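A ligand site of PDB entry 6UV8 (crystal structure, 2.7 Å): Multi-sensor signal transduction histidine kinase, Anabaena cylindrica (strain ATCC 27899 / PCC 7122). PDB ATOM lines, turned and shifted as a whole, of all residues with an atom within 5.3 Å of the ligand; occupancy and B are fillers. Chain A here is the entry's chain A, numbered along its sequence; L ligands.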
ATOM      1  N   ILE A  44     -15.083  -4.073  28.733  1.00  0.00           N
ATOM      2  CA  ILE A  44     -14.824  -2.831  29.424  1.00  0.00           C
ATOM      3  C   ILE A  44     -15.966  -1.864  29.181  1.00  0.00           C
ATOM      4  O   ILE A  44     -16.744  -2.014  28.235  1.00  0.00           O
ATOM      5  CB  ILE A  44     -13.468  -2.185  29.012  1.00  0.00           C
ATOM      6  CG1 ILE A  44     -13.471  -1.792  27.538  1.00  0.00           C
ATOM      7  CG2 ILE A  44     -12.315  -3.113  29.294  1.00  0.00           C
ATOM      8  CD1 ILE A  44     -13.388  -0.307  27.326  1.00  0.00           C
ATOM      9  N   PHE A  46     -15.665   1.928  28.649  1.00  0.00           N
ATOM     10  CA  PHE A  46     -14.824   3.115  28.506  1.00  0.00           C
ATOM     11  C   PHE A  46     -15.708   4.328  28.698  1.00  0.00           C
ATOM     12  O   PHE A  46     -16.614   4.572  27.906  1.00  0.00           O
ATOM     13  CB  PHE A  46     -14.148   3.142  27.142  1.00  0.00           C
ATOM     14  CG  PHE A  46     -13.042   4.117  27.045  1.00  0.00           C
ATOM     15  CD1 PHE A  46     -11.982   4.052  27.930  1.00  0.00           C
ATOM     16  CD2 PHE A  46     -13.056   5.109  26.088  1.00  0.00           C
ATOM     17  CE1 PHE A  46     -10.951   4.951  27.870  1.00  0.00           C
ATOM     18  CE2 PHE A  46     -12.028   6.012  26.014  1.00  0.00           C
ATOM     19  CZ  PHE A  46     -10.967   5.933  26.903  1.00  0.00           C
ATOM     20  N   SER A  54     -11.117  10.501  29.843  1.00  0.00           N
ATOM     21  CA  SER A  54     -11.800   9.268  29.513  1.00  0.00           C
ATOM     22  C   SER A  54     -11.117   8.136  30.252  1.00  0.00           C
ATOM     23  O   SER A  54      -9.898   8.159  30.437  1.00  0.00           O
ATOM     24  CB  SER A  54     -11.796   9.020  28.008  1.00  0.00           C
ATOM     25  OG  SER A  54     -10.494   9.074  27.459  1.00  0.00           O
ATOM     26  N   ILE A  56     -11.458   3.691  31.466  1.00  0.00           N
ATOM     27  CA  ILE A  56     -12.105   2.389  31.596  1.00  0.00           C
ATOM     28  C   ILE A  56     -12.584   2.256  33.040  1.00  0.00           C
ATOM     29  O   ILE A  56     -11.799   1.964  33.936  1.00  0.00           O
ATOM     30  CB  ILE A  56     -11.145   1.255  31.229  1.00  0.00           C
ATOM     31  CG1 ILE A  56     -10.734   1.375  29.778  1.00  0.00           C
ATOM     32  CG2 ILE A  56     -11.779  -0.077  31.468  1.00  0.00           C
ATOM     33  CD1 ILE A  56      -9.896   0.233  29.322  1.00  0.00           C
ATOM     34  N   TYR A  71      -7.820   2.453  33.307  1.00  0.00           N
ATOM     35  CA  TYR A  71      -7.014   3.001  32.220  1.00  0.00           C
ATOM     36  C   TYR A  71      -7.709   4.196  31.626  1.00  0.00           C
ATOM     37  O   TYR A  71      -8.928   4.214  31.461  1.00  0.00           O
ATOM     38  CB  TYR A  71      -6.734   1.938  31.160  1.00  0.00           C
ATOM     39  CG  TYR A  71      -5.454   2.180  30.428  1.00  0.00           C
ATOM     40  CD1 TYR A  71      -5.143   3.440  29.947  1.00  0.00           C
ATOM     41  CD2 TYR A  71      -4.530   1.163  30.252  1.00  0.00           C
ATOM     42  CE1 TYR A  71      -3.969   3.684  29.285  1.00  0.00           C
ATOM     43  CE2 TYR A  71      -3.334   1.399  29.582  1.00  0.00           C
ATOM     44  CZ  TYR A  71      -3.065   2.671  29.101  1.00  0.00           C
ATOM     45  OH  TYR A  71      -1.899   2.928  28.429  1.00  0.00           O
ATOM     46  N   HIS A  72      -6.938   5.224  31.327  1.00  0.00           N
ATOM     47  CA  HIS A  72      -7.500   6.557  31.232  1.00  0.00           C
ATOM     48  C   HIS A  72      -6.704   7.360  30.209  1.00  0.00           C
ATOM     49  O   HIS A  72      -5.731   6.868  29.631  1.00  0.00           O
ATOM     50  CB  HIS A  72      -7.483   7.254  32.596  1.00  0.00           C
ATOM     51  CG  HIS A  72      -6.140   7.273  33.272  1.00  0.00           C
ATOM     52  ND1 HIS A  72      -5.761   8.266  34.138  1.00  0.00           N
ATOM     53  CD2 HIS A  72      -5.094   6.407  33.205  1.00  0.00           C
ATOM     54  CE1 HIS A  72      -4.542   8.030  34.575  1.00  0.00           C
ATOM     55  NE2 HIS A  72      -4.116   6.904  34.028  1.00  0.00           N
ATOM     56  N   TRP A  73      -7.140   8.603  30.014  1.00  0.00           N
ATOM     57  CA  TRP A  73      -6.496   9.548  29.107  1.00  0.00           C
ATOM     58  C   TRP A  73      -7.278  10.862  29.085  1.00  0.00           C
ATOM     59  O   TRP A  73      -8.483  10.863  29.324  1.00  0.00           O
ATOM     60  CB  TRP A  73      -6.391   8.931  27.708  1.00  0.00           C
ATOM     61  CG  TRP A  73      -5.272   9.497  26.912  1.00  0.00           C
ATOM     62  CD1 TRP A  73      -3.942   9.232  27.049  1.00  0.00           C
ATOM     63  CD2 TRP A  73      -5.395  10.434  25.848  1.00  0.00           C
ATOM     64  NE1 TRP A  73      -3.219   9.966  26.126  1.00  0.00           N
ATOM     65  CE2 TRP A  73      -4.093  10.705  25.379  1.00  0.00           C
ATOM     66  CE3 TRP A  73      -6.492  11.067  25.241  1.00  0.00           C
ATOM     67  CZ2 TRP A  73      -3.851  11.595  24.327  1.00  0.00           C
ATOM     68  CZ3 TRP A  73      -6.246  11.940  24.206  1.00  0.00           C
ATOM     69  CH2 TRP A  73      -4.940  12.193  23.753  1.00  0.00           C
ATOM     70  N   ASP A  75      -8.160  14.762  27.096  1.00  0.00           N
ATOM     71  CA  ASP A  75      -8.311  15.427  25.791  1.00  0.00           C
ATOM     72  C   ASP A  75      -8.494  14.398  24.668  1.00  0.00           C
ATOM     73  O   ASP A  75      -7.773  14.407  23.668  1.00  0.00           O
ATOM     74  CB  ASP A  75      -7.144  16.371  25.491  1.00  0.00           C
ATOM     75  CG  ASP A  75      -7.411  17.304  24.299  1.00  0.00           C
ATOM     76  OD1 ASP A  75      -8.029  18.375  24.495  1.00  0.00           O
ATOM     77  OD2 ASP A  75      -6.986  16.985  23.173  1.00  0.00           O
ATOM     78  N   GLU A  76      -9.484  13.527  24.832  1.00  0.00           N
ATOM     79  CA  GLU A  76      -9.671  12.405  23.926  1.00  0.00           C
ATOM     80  C   GLU A  76     -10.396  12.877  22.676  1.00  0.00           C
ATOM     81  O   GLU A  76     -11.556  13.287  22.754  1.00  0.00           O
ATOM     82  CB  GLU A  76     -10.456  11.296  24.619  1.00  0.00           C
ATOM     83  CG  GLU A  76     -10.680  10.118  23.730  1.00  0.00           C
ATOM     84  CD  GLU A  76      -9.850   8.949  24.125  1.00  0.00           C
ATOM     85  OE1 GLU A  76      -9.478   8.883  25.314  1.00  0.00           O
ATOM     86  OE2 GLU A  76      -9.556   8.094  23.260  1.00  0.00           O
ATOM     87  N   LYS A  77      -9.735  12.803  21.531  1.00  0.00           N
ATOM     88  CA  LYS A  77     -10.313  13.191  20.251  1.00  0.00           C
ATOM     89  C   LYS A  77     -10.546  11.930  19.417  1.00  0.00           C
ATOM     90  O   LYS A  77      -9.605  11.174  19.168  1.00  0.00           O
ATOM     91  CB  LYS A  77      -9.396  14.169  19.497  1.00  0.00           C
ATOM     92  CG  LYS A  77      -9.637  15.646  19.789  1.00  0.00           C
ATOM     93  CD  LYS A  77      -8.427  16.506  19.429  1.00  0.00           C
ATOM     94  CE  LYS A  77      -8.601  17.950  19.929  1.00  0.00           C
ATOM     95  NZ  LYS A  77      -7.322  18.718  20.042  1.00  0.00           N
ATOM     96  N   TRP A  78     -11.783  11.712  19.004  1.00  0.00           N
ATOM     97  CA  TRP A  78     -12.079  10.602  18.118  1.00  0.00           C
ATOM     98  C   TRP A  78     -12.318  11.102  16.698  1.00  0.00           C
ATOM     99  O   TRP A  78     -12.788  12.216  16.489  1.00  0.00           O
ATOM    100  CB  TRP A  78     -13.308   9.823  18.577  1.00  0.00           C
ATOM    101  CG  TRP A  78     -13.036   8.967  19.721  1.00  0.00           C
ATOM    102  CD1 TRP A  78     -11.840   8.791  20.351  1.00  0.00           C
ATOM    103  CD2 TRP A  78     -13.979   8.163  20.419  1.00  0.00           C
ATOM    104  NE1 TRP A  78     -11.973   7.929  21.403  1.00  0.00           N
ATOM    105  CE2 TRP A  78     -13.285   7.529  21.463  1.00  0.00           C
ATOM    106  CE3 TRP A  78     -15.335   7.927  20.264  1.00  0.00           C
ATOM    107  CZ2 TRP A  78     -13.910   6.668  22.351  1.00  0.00           C
ATOM    108  CZ3 TRP A  78     -15.964   7.070  21.139  1.00  0.00           C
ATOM    109  CH2 TRP A  78     -15.248   6.441  22.171  1.00  0.00           C
ATOM    110  N   SER A  79     -11.998  10.247  15.734  1.00  0.00           N
ATOM    111  CA  SER A  79     -12.174  10.643  14.348  1.00  0.00           C
ATOM    112  C   SER A  79     -13.642  10.920  14.087  1.00  0.00           C
ATOM    113  O   SER A  79     -14.513  10.160  14.494  1.00  0.00           O
ATOM    114  CB  SER A  79     -11.637   9.568  13.410  1.00  0.00           C
ATOM    115  OG  SER A  79     -10.375   9.968  12.883  1.00  0.00           O
ATOM    116  N   ILE A  82     -16.185   8.560  12.864  1.00  0.00           N
ATOM    117  CA  ILE A  82     -16.436   7.461  13.781  1.00  0.00           C
ATOM    118  C   ILE A  82     -17.499   7.818  14.818  1.00  0.00           C
ATOM    119  O   ILE A  82     -18.309   6.973  15.191  1.00  0.00           O
ATOM    120  CB  ILE A  82     -15.105   7.051  14.463  1.00  0.00           C
ATOM    121  CG1 ILE A  82     -14.430   5.951  13.653  1.00  0.00           C
ATOM    122  CG2 ILE A  82     -15.308   6.640  15.891  1.00  0.00           C
ATOM    123  CD1 ILE A  82     -13.923   4.816  14.487  1.00  0.00           C
ATOM    124  N   TYR A  86     -21.211   6.479  15.717  1.00  0.00           N
ATOM    125  CA  TYR A  86     -21.563   6.159  17.107  1.00  0.00           C
ATOM    126  C   TYR A  86     -22.775   6.921  17.604  1.00  0.00           C
ATOM    127  O   TYR A  86     -23.561   6.394  18.408  1.00  0.00           O
ATOM    128  CB  TYR A  86     -20.384   6.421  18.047  1.00  0.00           C
ATOM    129  CG  TYR A  86     -19.319   5.341  18.026  1.00  0.00           C
ATOM    130  CD1 TYR A  86     -19.669   3.995  18.103  1.00  0.00           C
ATOM    131  CD2 TYR A  86     -17.978   5.667  17.922  1.00  0.00           C
ATOM    132  CE1 TYR A  86     -18.704   3.014  18.064  1.00  0.00           C
ATOM    133  CE2 TYR A  86     -17.011   4.695  17.892  1.00  0.00           C
ATOM    134  CZ  TYR A  86     -17.375   3.383  17.960  1.00  0.00           C
ATOM    135  OH  TYR A  86     -16.373   2.444  17.907  1.00  0.00           O
ATOM    136  N   ARG A  92     -19.707  -0.776  16.389  1.00  0.00           N
ATOM    137  CA  ARG A  92     -18.596  -0.798  15.429  1.00  0.00           C
ATOM    138  C   ARG A  92     -17.848  -2.109  15.560  1.00  0.00           C
ATOM    139  O   ARG A  92     -17.296  -2.411  16.628  1.00  0.00           O
ATOM    140  CB  ARG A  92     -17.645   0.376  15.648  1.00  0.00           C
ATOM    141  CG  ARG A  92     -16.521   0.432  14.647  1.00  0.00           C
ATOM    142  CD  ARG A  92     -15.770   1.716  14.773  1.00  0.00           C
ATOM    143  NE  ARG A  92     -14.424   1.526  15.279  1.00  0.00           N
ATOM    144  CZ  ARG A  92     -13.371   1.235  14.516  1.00  0.00           C
ATOM    145  NH1 ARG A  92     -12.181   1.082  15.062  1.00  0.00           N
ATOM    146  NH2 ARG A  92     -13.515   1.082  13.204  1.00  0.00           N
ATOM    147  N   VAL A  94     -14.720  -4.265  14.813  1.00  0.00           N
ATOM    148  CA  VAL A  94     -13.301  -4.082  14.521  1.00  0.00           C
ATOM    149  C   VAL A  94     -12.743  -5.495  14.432  1.00  0.00           C
ATOM    150  O   VAL A  94     -12.288  -6.041  15.456  1.00  0.00           O
ATOM    151  CB  VAL A  94     -12.642  -3.235  15.607  1.00  0.00           C
ATOM    152  CG1 VAL A  94     -11.499  -2.403  15.059  1.00  0.00           C
ATOM    153  CG2 VAL A  94     -13.709  -2.362  16.248  1.00  0.00           C
ATOM    154  N   ASP A 100      -6.554  -1.491  12.396  1.00  0.00           N
ATOM    155  CA  ASP A 100      -7.671  -0.551  12.429  1.00  0.00           C
ATOM    156  C   ASP A 100      -7.118   0.862  12.451  1.00  0.00           C
ATOM    157  O   ASP A 100      -6.617   1.311  13.473  1.00  0.00           O
ATOM    158  CB  ASP A 100      -8.548  -0.796  13.640  1.00  0.00           C
ATOM    159  CG  ASP A 100      -9.620   0.216  13.742  1.00  0.00           C
ATOM    160  OD1 ASP A 100     -10.286   0.464  12.722  1.00  0.00           O
ATOM    161  OD2 ASP A 100      -9.786   0.804  14.828  1.00  0.00           O
ATOM    162  N   ILE A 101      -7.236   1.565  11.324  1.00  0.00           N
ATOM    163  CA  ILE A 101      -6.627   2.875  11.208  1.00  0.00           C
ATOM    164  C   ILE A 101      -7.234   3.883  12.193  1.00  0.00           C
ATOM    165  O   ILE A 101      -6.595   4.887  12.521  1.00  0.00           O
ATOM    166  CB  ILE A 101      -6.730   3.342   9.739  1.00  0.00           C
ATOM    167  CG1 ILE A 101      -5.843   4.549   9.482  1.00  0.00           C
ATOM    168  CG2 ILE A 101      -8.162   3.654   9.370  1.00  0.00           C
ATOM    169  CD1 ILE A 101      -4.390   4.209   9.401  1.00  0.00           C
ATOM    170  N   TRP A 102      -8.432   3.616  12.710  1.00  0.00           N
ATOM    171  CA  TRP A 102      -9.072   4.562  13.625  1.00  0.00           C
ATOM    172  C   TRP A 102      -8.549   4.416  15.045  1.00  0.00           C
ATOM    173  O   TRP A 102      -8.666   5.342  15.857  1.00  0.00           O
ATOM    174  CB  TRP A 102     -10.588   4.363  13.580  1.00  0.00           C
ATOM    175  CG  TRP A 102     -11.077   4.230  12.175  1.00  0.00           C
ATOM    176  CD1 TRP A 102     -11.255   3.070  11.469  1.00  0.00           C
ATOM    177  CD2 TRP A 102     -11.414   5.282  11.282  1.00  0.00           C
ATOM    178  NE1 TRP A 102     -11.681   3.346  10.197  1.00  0.00           N
ATOM    179  CE2 TRP A 102     -11.788   4.705  10.056  1.00  0.00           C
ATOM    180  CE3 TRP A 102     -11.447   6.679  11.399  1.00  0.00           C
ATOM    181  CZ2 TRP A 102     -12.179   5.467   8.979  1.00  0.00           C
ATOM    182  CZ3 TRP A 102     -11.833   7.420  10.322  1.00  0.00           C
ATOM    183  CH2 TRP A 102     -12.198   6.821   9.125  1.00  0.00           C
ATOM    184  N   THR A 103      -7.986   3.251  15.349  1.00  0.00           N
ATOM    185  CA  THR A 103      -7.389   2.887  16.631  1.00  0.00           C
ATOM    186  C   THR A 103      -5.900   2.643  16.422  1.00  0.00           C
ATOM    187  O   THR A 103      -5.306   1.740  17.017  1.00  0.00           O
ATOM    188  CB  THR A 103      -8.120   1.662  17.159  1.00  0.00           C
ATOM    189  OG1 THR A 103      -9.509   1.969  17.151  1.00  0.00           O
ATOM    190  CG2 THR A 103      -7.744   1.301  18.573  1.00  0.00           C
ATOM    191  N   SER A 104      -5.293   3.425  15.516  1.00  0.00           N
ATOM    192  CA  SER A 104      -3.876   3.294  15.162  1.00  0.00           C
ATOM    193  C   SER A 104      -2.984   3.997  16.162  1.00  0.00           C
ATOM    194  O   SER A 104      -1.769   4.040  15.979  1.00  0.00           O
ATOM    195  CB  SER A 104      -3.619   3.844  13.752  1.00  0.00           C
ATOM    196  OG  SER A 104      -3.309   5.233  13.745  1.00  0.00           O
ATOM    197  N   CYS A 105      -3.579   4.558  17.195  1.00  0.00           N
ATOM    198  CA  CYS A 105      -2.858   5.172  18.294  1.00  0.00           C
ATOM    199  C   CYS A 105      -2.919   4.349  19.574  1.00  0.00           C
ATOM    200  O   CYS A 105      -2.003   4.440  20.394  1.00  0.00           O
ATOM    201  CB  CYS A 105      -3.430   6.555  18.561  1.00  0.00           C
ATOM    202  SG  CYS A 105      -5.206   6.524  18.465  1.00  0.00           S
ATOM    203  N   LEU A 106      -3.975   3.570  19.777  1.00  0.00           N
ATOM    204  CA  LEU A 106      -4.050   2.658  20.905  1.00  0.00           C
ATOM    205  C   LEU A 106      -3.297   1.375  20.554  1.00  0.00           C
ATOM    206  O   LEU A 106      -3.860   0.290  20.471  1.00  0.00           O
ATOM    207  CB  LEU A 106      -5.486   2.330  21.266  1.00  0.00           C
ATOM    208  CG  LEU A 106      -6.497   3.450  21.138  1.00  0.00           C
ATOM    209  CD1 LEU A 106      -7.793   2.938  21.695  1.00  0.00           C
ATOM    210  CD2 LEU A 106      -6.039   4.656  21.899  1.00  0.00           C
ATOM    211  N   GLU A 108      -0.132   0.930  22.245  1.00  0.00           N
ATOM    212  CA  GLU A 108       0.233   0.632  23.620  1.00  0.00           C
ATOM    213  C   GLU A 108      -0.918  -0.143  24.225  1.00  0.00           C
ATOM    214  O   GLU A 108      -0.777  -1.320  24.563  1.00  0.00           O
ATOM    215  CB  GLU A 108       0.479   1.929  24.392  1.00  0.00           C
ATOM    216  CG  GLU A 108      -0.478   3.063  24.039  1.00  0.00           C
ATOM    217  CD  GLU A 108      -0.367   4.262  24.950  1.00  0.00           C
ATOM    218  OE1 GLU A 108       0.498   5.115  24.687  1.00  0.00           O
ATOM    219  OE2 GLU A 108      -1.153   4.361  25.932  1.00  0.00           O
ATOM    220  N   TYR A 109      -2.065   0.529  24.302  1.00  0.00           N
ATOM    221  CA  TYR A 109      -3.248  -0.041  24.916  1.00  0.00           C
ATOM    222  C   TYR A 109      -3.601  -1.375  24.294  1.00  0.00           C
ATOM    223  O   TYR A 109      -3.943  -2.328  24.997  1.00  0.00           O
ATOM    224  CB  TYR A 109      -4.393   0.959  24.784  1.00  0.00           C
ATOM    225  CG  TYR A 109      -5.722   0.427  25.207  1.00  0.00           C
ATOM    226  CD1 TYR A 109      -6.100   0.435  26.541  1.00  0.00           C
ATOM    227  CD2 TYR A 109      -6.624  -0.071  24.270  1.00  0.00           C
ATOM    228  CE1 TYR A 109      -7.328  -0.060  26.938  1.00  0.00           C
ATOM    229  CE2 TYR A 109      -7.857  -0.548  24.651  1.00  0.00           C
ATOM    230  CZ  TYR A 109      -8.194  -0.539  25.982  1.00  0.00           C
ATOM    231  OH  TYR A 109      -9.425  -1.020  26.345  1.00  0.00           O
ATOM    232  N   ILE A 115      -5.473  -7.241  22.507  1.00  0.00           N
ATOM    233  CA  ILE A 115      -6.758  -7.300  21.802  1.00  0.00           C
ATOM    234  C   ILE A 115      -6.543  -7.654  20.343  1.00  0.00           C
ATOM    235  O   ILE A 115      -5.792  -6.985  19.622  1.00  0.00           O
ATOM    236  CB  ILE A 115      -7.494  -5.962  21.897  1.00  0.00           C
ATOM    237  CG1 ILE A 115      -7.456  -5.404  23.313  1.00  0.00           C
ATOM    238  CG2 ILE A 115      -8.918  -6.121  21.356  1.00  0.00           C
ATOM    239  CD1 ILE A 115      -7.493  -3.899  23.333  1.00  0.00           C
ATOM    240  N   LYS A 118     -12.591  -6.790  18.189  1.00  0.00           N
ATOM    241  CA  LYS A 118     -13.473  -6.235  19.210  1.00  0.00           C
ATOM    242  C   LYS A 118     -14.747  -5.686  18.576  1.00  0.00           C
ATOM    243  O   LYS A 118     -14.768  -5.341  17.392  1.00  0.00           O
ATOM    244  CB  LYS A 118     -12.779  -5.133  20.018  1.00  0.00           C
ATOM    245  CG  LYS A 118     -12.348  -3.973  19.182  1.00  0.00           C
ATOM    246  CD  LYS A 118     -12.233  -2.674  19.939  1.00  0.00           C
ATOM    247  CE  LYS A 118     -11.647  -1.646  18.997  1.00  0.00           C
ATOM    248  NZ  LYS A 118     -10.740  -0.636  19.609  1.00  0.00           N
ATOM    249  N   VAL A 120     -17.409  -2.519  19.489  1.00  0.00           N
ATOM    250  CA  VAL A 120     -17.515  -1.260  20.229  1.00  0.00           C
ATOM    251  C   VAL A 120     -18.956  -0.770  20.144  1.00  0.00           C
ATOM    252  O   VAL A 120     -19.495  -0.621  19.043  1.00  0.00           O
ATOM    253  CB  VAL A 120     -16.563  -0.210  19.639  1.00  0.00           C
ATOM    254  CG1 VAL A 120     -16.650   1.026  20.427  1.00  0.00           C
ATOM    255  CG2 VAL A 120     -15.168  -0.728  19.590  1.00  0.00           C
ATOM    256  N   VAL A 149     -17.326  -2.036  25.298  1.00  0.00           N
ATOM    257  CA  VAL A 149     -16.454  -2.743  24.372  1.00  0.00           C
ATOM    258  C   VAL A 149     -16.318  -4.192  24.822  1.00  0.00           C
ATOM    259  O   VAL A 149     -16.446  -4.518  26.009  1.00  0.00           O
ATOM    260  CB  VAL A 149     -15.059  -2.092  24.241  1.00  0.00           C
ATOM    261  CG1 VAL A 149     -14.291  -2.665  23.056  1.00  0.00           C
ATOM    262  CG2 VAL A 149     -15.186  -0.628  24.092  1.00  0.00           C
ATOM    263  N   HIS A 151     -13.670  -7.563  23.945  1.00  0.00           N
ATOM    264  CA  HIS A 151     -12.326  -7.789  23.400  1.00  0.00           C
ATOM    265  C   HIS A 151     -12.084  -9.280  23.112  1.00  0.00           C
ATOM    266  O   HIS A 151     -11.941 -10.074  24.037  1.00  0.00           O
ATOM    267  CB  HIS A 151     -11.240  -7.293  24.368  1.00  0.00           C
ATOM    268  CG  HIS A 151     -11.114  -5.806  24.450  1.00  0.00           C
ATOM    269  ND1 HIS A 151     -10.596  -5.169  25.553  1.00  0.00           N
ATOM    270  CD2 HIS A 151     -11.425  -4.831  23.566  1.00  0.00           C
ATOM    271  CE1 HIS A 151     -10.597  -3.864  25.343  1.00  0.00           C
ATOM    272  NE2 HIS A 151     -11.096  -3.633  24.147  1.00  0.00           N
HETATM  273  C1  LIG L   1     -11.141   4.623  22.397  1.00  0.00           C
HETATM  274  N1  LIG L   1      -9.266   5.464  23.699  1.00  0.00           N
HETATM  275  C2  LIG L   1     -10.230   4.567  23.389  1.00  0.00           C
HETATM  276  C3  LIG L   1     -10.157   3.547  24.243  1.00  0.00           C
HETATM  277  C4  LIG L   1      -9.164   3.794  25.079  1.00  0.00           C
HETATM  278  C5  LIG L   1      -8.606   4.946  24.748  1.00  0.00           C
HETATM  279  C6  LIG L   1      -8.719   2.882  26.219  1.00  0.00           C
HETATM  280  C7  LIG L   1     -10.997   2.287  24.326  1.00  0.00           C
HETATM  281  C8  LIG L   1     -10.355   1.282  23.378  1.00  0.00           C
HETATM  282  C9  LIG L   1     -11.090  -0.043  23.495  1.00  0.00           C
HETATM  283  O1  LIG L   1     -11.369  -0.404  24.638  1.00  0.00           O
HETATM  284  O2  LIG L   1     -11.319  -0.697  22.457  1.00  0.00           O
HETATM  285  C10 LIG L   1      -7.594   5.454  25.457  1.00  0.00           C
HETATM  286  N2  LIG L   1      -6.810   7.102  23.922  1.00  0.00           N
HETATM  287  C11 LIG L   1      -6.635   6.159  24.855  1.00  0.00           C
HETATM  288  C12 LIG L   1      -5.324   6.053  25.113  1.00  0.00           C
HETATM  289  C13 LIG L   1      -4.701   6.920  24.342  1.00  0.00           C
HETATM  290  C14 LIG L   1      -5.596   7.564  23.604  1.00  0.00           C
HETATM  291  C15 LIG L   1      -4.639   5.106  26.105  1.00  0.00           C
HETATM  292  C16 LIG L   1      -3.384   7.108  24.280  1.00  0.00           C
HETATM  293  C17 LIG L   1      -2.794   6.643  22.956  1.00  0.00           C
HETATM  294  O3  LIG L   1      -5.380   8.547  22.670  1.00  0.00           O
HETATM  295  N3  LIG L   1      -8.482   8.394  20.478  1.00  0.00           N
HETATM  296  C18 LIG L   1      -7.741   9.507  20.656  1.00  0.00           C
HETATM  297  C19 LIG L   1      -6.703   9.677  19.545  1.00  0.00           C
HETATM  298  C20 LIG L   1      -6.972   8.477  18.670  1.00  0.00           C
HETATM  299  C21 LIG L   1      -8.108   7.719  19.368  1.00  0.00           C
HETATM  300  C22 LIG L   1      -6.484  11.045  18.930  1.00  0.00           C
HETATM  301  C23 LIG L   1      -5.891   7.858  17.779  1.00  0.00           C
HETATM  302  C24 LIG L   1      -6.242   8.005  16.287  1.00  0.00           C
HETATM  303  O4  LIG L   1      -7.890  10.292  21.589  1.00  0.00           O
HETATM  304  C25 LIG L   1      -8.652   6.581  18.912  1.00  0.00           C
HETATM  305  N4  LIG L   1      -9.586   5.667  20.898  1.00  0.00           N
HETATM  306  C26 LIG L   1      -9.638   6.006  19.606  1.00  0.00           C
HETATM  307  C27 LIG L   1     -10.819   5.642  19.119  1.00  0.00           C
HETATM  308  C28 LIG L   1     -11.517   5.070  20.105  1.00  0.00           C
HETATM  309  C29 LIG L   1     -10.773   5.138  21.205  1.00  0.00           C
HETATM  310  C30 LIG L   1     -11.260   5.852  17.670  1.00  0.00           C
HETATM  311  C31 LIG L   1     -12.976   4.515  20.138  1.00  0.00           C
HETATM  312  C32 LIG L   1     -13.283   3.012  20.095  1.00  0.00           C
HETATM  313  C33 LIG L   1     -12.923   2.271  18.809  1.00  0.00           C
HETATM  314  O5  LIG L   1     -13.508   2.652  17.774  1.00  0.00           O
HETATM  315  O6  LIG L   1     -12.178   1.279  18.906  1.00  0.00           O
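A carbon (C23) of the ligand is bonded to the side-chain sulfur (SG) of Cys 105 (1.6 Å). An oxygen (O6) of the ligand lies within salt-bridge range of the side-chain amino group of Lys 118 (2.5 Å). An oxygen (O1) of the ligand is in hydrogen-bond range of the side-chain hydroxyl (OH) of Tyr 109 (2.7 Å). A nitrogen (N1) of the ligand lies within hydrogen-bond range of the side-chain carboxylate of Glu 76 (2.7 Å). O5 of the ligand sits at hydrogen-bond distance from OH of Tyr 86, at 2.9 Å. The guanidinium group (NE) of Arg 92 lies within salt-bridge range of an oxygen (O5) of the ligand (2.9 Å). The backbone NH of Lys 77 lies within hydrogen-bond range of an oxygen (O4) of the ligand. N3 of the ligand sits close to O of Lys 77 (3.3 Å). The side-chain hydroxyl (OG1) of Thr 103 lies within hydrogen-bond range of an oxygen (O6) of the ligand. A ring nitrogen (NE2) of His 151 lies within hydrogen-bond range of an oxygen (O1) of the ligand (3.3 Å).
The backbone NH (N) of Val 94 sits at hydrogen-bond distance from the backbone carbonyl oxygen (O) of Lys 118 (2.8 Å). The guanidinium group (NE) of Arg 92 lies close to the side-chain hydroxyl (OH) of Tyr 86. The backbone NH (N) of Arg 92 lies within hydrogen-bond range of the backbone carbonyl oxygen (O) of Val 120, 2.7 Å away. The side-chain carboxylate (OD2) of Asp 100 is in salt-bridge range of the guanidinium group (NH1) of Arg 92, 2.4 Å away. The side-chain amino group (NZ) of Lys 77 lies within salt-bridge range of the side-chain carboxylate (OD2) of Asp 75. N of Val 149 lies within hydrogen-bond range of O of Ile 44 (3.0 Å). The backbone NH (N) of Ser 54 lies within hydrogen-bond range of the backbone carbonyl oxygen (O) of Trp 73, 2.7 Å away. The backbone NH (N) of Ile 56 is in hydrogen-bond range of the backbone carbonyl oxygen (O) of Tyr 71 (2.6 Å).
NE1 of Trp 78 sits close to N4 of the ligand (3.3 Å). CD1 of Ile 44 touches O1 of the ligand, at 3.4 Å. CZ of Phe 46 touches C4 of the ligand, at 3.3 Å. Tyr 71 touches the ligand (CE1 to C15, 3.5 Å). NE1 of Trp 73 touches C16 of the ligand, at 3.4 Å. CD1 of Ile 82 touches O5 of the ligand, 3.96 Å away. O of Trp 102 touches C30 of the ligand, 3.2 Å away. Leu 106 touches the ligand. Glu 108 touches the ligand (OE2 to C15, 3.6 Å). Val 120 touches the ligand. CG1 of Val 149 touches O2 of the ligand, at 3.6 Å. Hydrophobic or aromatic side chains that line the ligand: Ile 44, Phe 46, Tyr 71, Trp 73, Trp 78, Ile 82, Tyr 86, Leu 106, Tyr 109, Val 120, Val 149 and His 151. The nearest printed residue that does not touch the ligand is His 72 (4.1 Å).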
